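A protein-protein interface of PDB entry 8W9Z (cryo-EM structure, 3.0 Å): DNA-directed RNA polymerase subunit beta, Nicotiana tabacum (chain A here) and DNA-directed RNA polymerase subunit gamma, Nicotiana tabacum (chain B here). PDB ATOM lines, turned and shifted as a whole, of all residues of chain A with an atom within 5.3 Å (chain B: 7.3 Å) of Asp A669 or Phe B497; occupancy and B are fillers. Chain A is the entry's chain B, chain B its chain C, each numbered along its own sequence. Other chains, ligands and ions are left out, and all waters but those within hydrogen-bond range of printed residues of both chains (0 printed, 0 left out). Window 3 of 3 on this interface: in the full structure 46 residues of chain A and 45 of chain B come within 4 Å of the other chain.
Printed residues of chain A that touch a printed residue of chain B: Asp A669, Lys A819, Lys A827 and Ile A829. Hydrophobic or aromatic side chains of chain B within 4 Å of the printed part of chain A: Phe B497. Among the printed residues, no Asp or Glu carboxylate lies within 4 Å of a Lys or Arg side-chain nitrogen of the other chain.
Among the printed residues, merely in contact across the chains: Asp A669 with Phe B497, Lys A827 with Phe B497, Lys A819 with Gly B499, Lys A827 with Asp B498, Lys A819 with Asp B498 and Ile A829 with Phe B497.
The backbone carbonyl oxygen of Ile A829 is in hydrogen-bond range of the backbone NH of Val A671 (3.1 Å).
Of chain A, only Asp A669, Lys A827 and Ile A829 come within 4 Å of Phe B497. Printed residues of chain A within 4 Å of Asp B498: Lys A819 (3.8 Å) and Lys A827 (3.7 Å). Of the printed residues of chain B, Lys A827 touches Phe B497 (3.6 Å) and Asp B498 (3.7 Å). Ser A667 touches none of the printed residues of chain B. Ala B495 touches none of the printed residues of chain A.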
ATOM      1  N   ASN A 666      30.988   4.400  31.372  1.00  0.00           N
ATOM      2  CA  ASN A 666      30.543   5.127  30.192  1.00  0.00           C
ATOM      3  C   ASN A 666      31.505   4.905  29.034  1.00  0.00           C
ATOM      4  O   ASN A 666      31.796   5.821  28.259  1.00  0.00           O
ATOM      5  CB  ASN A 666      30.385   6.615  30.493  1.00  0.00           C
ATOM      6  CG  ASN A 666      31.600   7.206  31.176  1.00  0.00           C
ATOM      7  OD1 ASN A 666      31.675   7.245  32.405  1.00  0.00           O
ATOM      8  ND2 ASN A 666      32.559   7.671  30.385  1.00  0.00           N
ATOM      9  N   SER A 667      32.025   3.681  28.906  1.00  0.00           N
ATOM     10  CA  SER A 667      32.858   3.350  27.754  1.00  0.00           C
ATOM     11  C   SER A 667      32.065   3.487  26.461  1.00  0.00           C
ATOM     12  O   SER A 667      32.492   4.169  25.522  1.00  0.00           O
ATOM     13  CB  SER A 667      33.416   1.934  27.898  1.00  0.00           C
ATOM     14  OG  SER A 667      32.374   0.973  27.901  1.00  0.00           O
ATOM     15  N   GLU A 668      30.904   2.844  26.396  1.00  0.00           N
ATOM     16  CA  GLU A 668      29.952   3.080  25.326  1.00  0.00           C
ATOM     17  C   GLU A 668      29.135   4.329  25.648  1.00  0.00           C
ATOM     18  O   GLU A 668      29.460   5.100  26.556  1.00  0.00           O
ATOM     19  CB  GLU A 668      29.053   1.860  25.137  1.00  0.00           C
ATOM     20  N   ASP A 669      28.059   4.541  24.900  1.00  0.00           N
ATOM     21  CA  ASP A 669      27.138   5.628  25.211  1.00  0.00           C
ATOM     22  C   ASP A 669      26.357   5.265  26.468  1.00  0.00           C
ATOM     23  O   ASP A 669      25.382   4.510  26.406  1.00  0.00           O
ATOM     24  CB  ASP A 669      26.203   5.891  24.034  1.00  0.00           C
ATOM     25  CG  ASP A 669      26.946   6.345  22.793  1.00  0.00           C
ATOM     26  OD1 ASP A 669      28.195   6.332  22.808  1.00  0.00           O
ATOM     27  OD2 ASP A 669      26.283   6.721  21.805  1.00  0.00           O
ATOM     28  N   ALA A 670      26.787   5.798  27.608  1.00  0.00           N
ATOM     29  CA  ALA A 670      26.174   5.473  28.887  1.00  0.00           C
ATOM     30  C   ALA A 670      26.402   6.630  29.847  1.00  0.00           C
ATOM     31  O   ALA A 670      27.371   7.381  29.715  1.00  0.00           O
ATOM     32  CB  ALA A 670      26.739   4.173  29.467  1.00  0.00           C
ATOM     33  N   VAL A 671      25.495   6.765  30.812  1.00  0.00           N
ATOM     34  CA  VAL A 671      25.508   7.872  31.759  1.00  0.00           C
ATOM     35  C   VAL A 671      25.543   7.316  33.174  1.00  0.00           C
ATOM     36  O   VAL A 671      24.811   6.374  33.500  1.00  0.00           O
ATOM     37  CB  VAL A 671      24.286   8.795  31.568  1.00  0.00           C
ATOM     38  CG1 VAL A 671      24.396  10.019  32.463  1.00  0.00           C
ATOM     39  CG2 VAL A 671      24.150   9.206  30.111  1.00  0.00           C
ATOM     40  N   LYS A 819      16.653   5.576  29.465  1.00  0.00           N
ATOM     41  CA  LYS A 819      17.371   6.290  28.419  1.00  0.00           C
ATOM     42  C   LYS A 819      17.144   7.787  28.583  1.00  0.00           C
ATOM     43  O   LYS A 819      16.000   8.251  28.568  1.00  0.00           O
ATOM     44  CB  LYS A 819      16.918   5.826  27.035  1.00  0.00           C
ATOM     45  CG  LYS A 819      17.191   4.360  26.754  1.00  0.00           C
ATOM     46  CD  LYS A 819      16.692   3.961  25.376  1.00  0.00           C
ATOM     47  CE  LYS A 819      17.352   4.790  24.289  1.00  0.00           C
ATOM     48  NZ  LYS A 819      16.870   4.412  22.933  1.00  0.00           N
ATOM     49  N   LYS A 827      22.690  10.541  23.289  1.00  0.00           N
ATOM     50  CA  LYS A 827      21.839   9.528  23.894  1.00  0.00           C
ATOM     51  C   LYS A 827      22.667   8.685  24.850  1.00  0.00           C
ATOM     52  O   LYS A 827      23.808   8.325  24.544  1.00  0.00           O
ATOM     53  CB  LYS A 827      21.194   8.634  22.826  1.00  0.00           C
ATOM     54  CG  LYS A 827      20.258   7.574  23.378  1.00  0.00           C
ATOM     55  CD  LYS A 827      19.819   6.604  22.292  1.00  0.00           C
ATOM     56  CE  LYS A 827      19.077   7.319  21.176  1.00  0.00           C
ATOM     57  NZ  LYS A 827      18.646   6.379  20.103  1.00  0.00           N
ATOM     58  N   GLY A 828      22.092   8.375  26.008  1.00  0.00           N
ATOM     59  CA  GLY A 828      22.793   7.587  27.000  1.00  0.00           C
ATOM     60  C   GLY A 828      21.883   6.715  27.837  1.00  0.00           C
ATOM     61  O   GLY A 828      20.766   7.115  28.177  1.00  0.00           O
ATOM     62  N   ILE A 829      22.352   5.517  28.174  1.00  0.00           N
ATOM     63  CA  ILE A 829      21.619   4.581  29.017  1.00  0.00           C
ATOM     64  C   ILE A 829      22.254   4.596  30.399  1.00  0.00           C
ATOM     65  O   ILE A 829      23.479   4.491  30.527  1.00  0.00           O
ATOM     66  CB  ILE A 829      21.620   3.162  28.422  1.00  0.00           C
ATOM     67  CG1 ILE A 829      21.105   3.189  26.982  1.00  0.00           C
ATOM     68  CG2 ILE A 829      20.769   2.230  29.267  1.00  0.00           C
ATOM     69  CD1 ILE A 829      21.066   1.827  26.324  1.00  0.00           C
ATOM     70  N   ILE B 391      20.577  -3.549  27.322  1.00  0.00           N
ATOM     71  CA  ILE B 391      21.861  -4.041  27.802  1.00  0.00           C
ATOM     72  C   ILE B 391      22.719  -2.851  28.210  1.00  0.00           C
ATOM     73  O   ILE B 391      22.835  -1.875  27.459  1.00  0.00           O
ATOM     74  CB  ILE B 391      22.576  -4.900  26.742  1.00  0.00           C
ATOM     75  CG1 ILE B 391      22.550  -4.207  25.378  1.00  0.00           C
ATOM     76  CG2 ILE B 391      21.937  -6.276  26.658  1.00  0.00           C
ATOM     77  CD1 ILE B 391      23.243  -4.986  24.283  1.00  0.00           C
ATOM     78  N   VAL B 393      26.581  -1.635  30.279  1.00  0.00           N
ATOM     79  CA  VAL B 393      27.982  -2.028  30.377  1.00  0.00           C
ATOM     80  C   VAL B 393      28.341  -2.188  31.848  1.00  0.00           C
ATOM     81  O   VAL B 393      28.164  -1.259  32.647  1.00  0.00           O
ATOM     82  CB  VAL B 393      28.901  -1.010  29.684  1.00  0.00           C
ATOM     83  CG1 VAL B 393      28.883  -1.224  28.180  1.00  0.00           C
ATOM     84  CG2 VAL B 393      28.473   0.411  30.018  1.00  0.00           C
ATOM     85  N   ASN B 494      28.519  -5.568  18.318  1.00  0.00           N
ATOM     86  CA  ASN B 494      27.967  -4.405  17.621  1.00  0.00           C
ATOM     87  C   ASN B 494      26.968  -3.655  18.505  1.00  0.00           C
ATOM     88  O   ASN B 494      25.777  -3.552  18.204  1.00  0.00           O
ATOM     89  CB  ASN B 494      27.330  -4.815  16.288  1.00  0.00           C
ATOM     90  N   ALA B 495      27.481  -3.131  19.616  1.00  0.00           N
ATOM     91  CA  ALA B 495      26.653  -2.357  20.530  1.00  0.00           C
ATOM     92  C   ALA B 495      26.256  -1.030  19.898  1.00  0.00           C
ATOM     93  O   ALA B 495      27.037  -0.410  19.169  1.00  0.00           O
ATOM     94  CB  ALA B 495      27.392  -2.114  21.845  1.00  0.00           C
ATOM     95  N   ASP B 496      25.032  -0.592  20.182  1.00  0.00           N
ATOM     96  CA  ASP B 496      24.490   0.640  19.635  1.00  0.00           C
ATOM     97  C   ASP B 496      24.172   1.617  20.759  1.00  0.00           C
ATOM     98  O   ASP B 496      24.097   1.247  21.934  1.00  0.00           O
ATOM     99  CB  ASP B 496      23.222   0.375  18.811  1.00  0.00           C
ATOM    100  CG  ASP B 496      23.426  -0.685  17.748  1.00  0.00           C
ATOM    101  OD1 ASP B 496      24.564  -0.830  17.258  1.00  0.00           O
ATOM    102  OD2 ASP B 496      22.440  -1.371  17.402  1.00  0.00           O
ATOM    103  N   PHE B 497      23.987   2.883  20.378  1.00  0.00           N
ATOM    104  CA  PHE B 497      23.563   3.890  21.346  1.00  0.00           C
ATOM    105  C   PHE B 497      22.153   3.606  21.848  1.00  0.00           C
ATOM    106  O   PHE B 497      21.868   3.753  23.042  1.00  0.00           O
ATOM    107  CB  PHE B 497      23.642   5.283  20.722  1.00  0.00           C
ATOM    108  N   ASP B 498      21.260   3.203  20.949  1.00  0.00           N
ATOM    109  CA  ASP B 498      19.903   2.850  21.331  1.00  0.00           C
ATOM    110  C   ASP B 498      19.890   1.553  22.136  1.00  0.00           C
ATOM    111  O   ASP B 498      20.851   0.778  22.138  1.00  0.00           O
ATOM    112  CB  ASP B 498      19.019   2.705  20.092  1.00  0.00           C
ATOM    113  CG  ASP B 498      19.721   1.979  18.960  1.00  0.00           C
ATOM    114  OD1 ASP B 498      20.797   2.447  18.534  1.00  0.00           O
ATOM    115  OD2 ASP B 498      19.205   0.937  18.503  1.00  0.00           O
ATOM    116  N   GLY B 499      18.776   1.323  22.826  1.00  0.00           N
ATOM    117  CA  GLY B 499      18.608   0.108  23.597  1.00  0.00           C
ATOM    118  C   GLY B 499      18.499  -1.125  22.726  1.00  0.00           C
ATOM    119  O   GLY B 499      17.492  -1.322  22.039  1.00  0.00           O
ATOM    120  N   ASP B 500      19.531  -1.964  22.744  1.00  0.00           N
ATOM    121  CA  ASP B 500      19.559  -3.179  21.940  1.00  0.00           C
ATOM    122  C   ASP B 500      18.907  -4.312  22.722  1.00  0.00           C
ATOM    123  O   ASP B 500      19.372  -4.671  23.809  1.00  0.00           O
ATOM    124  CB  ASP B 500      20.994  -3.540  21.556  1.00  0.00           C
ATOM    125  CG  ASP B 500      21.663  -2.464  20.723  1.00  0.00           C
ATOM    126  OD1 ASP B 500      20.954  -1.773  19.959  1.00  0.00           O
ATOM    127  OD2 ASP B 500      22.898  -2.308  20.831  1.00  0.00           O
ATOM    128  N   GLN B 540      37.324   2.075  23.143  1.00  0.00           N
ATOM    129  CA  GLN B 540      37.809   3.448  23.045  1.00  0.00           C
ATOM    130  C   GLN B 540      38.470   3.902  24.342  1.00  0.00           C
ATOM    131  O   GLN B 540      39.594   4.419  24.333  1.00  0.00           O
ATOM    132  CB  GLN B 540      36.652   4.377  22.679  1.00  0.00           C
ATOM    133  CG  GLN B 540      35.805   3.887  21.517  1.00  0.00           C
ATOM    134  CD  GLN B 540      34.641   4.810  21.217  1.00  0.00           C
ATOM    135  OE1 GLN B 540      34.453   5.829  21.882  1.00  0.00           O
ATOM    136  NE2 GLN B 540      33.849   4.455  20.211  1.00  0.00           N
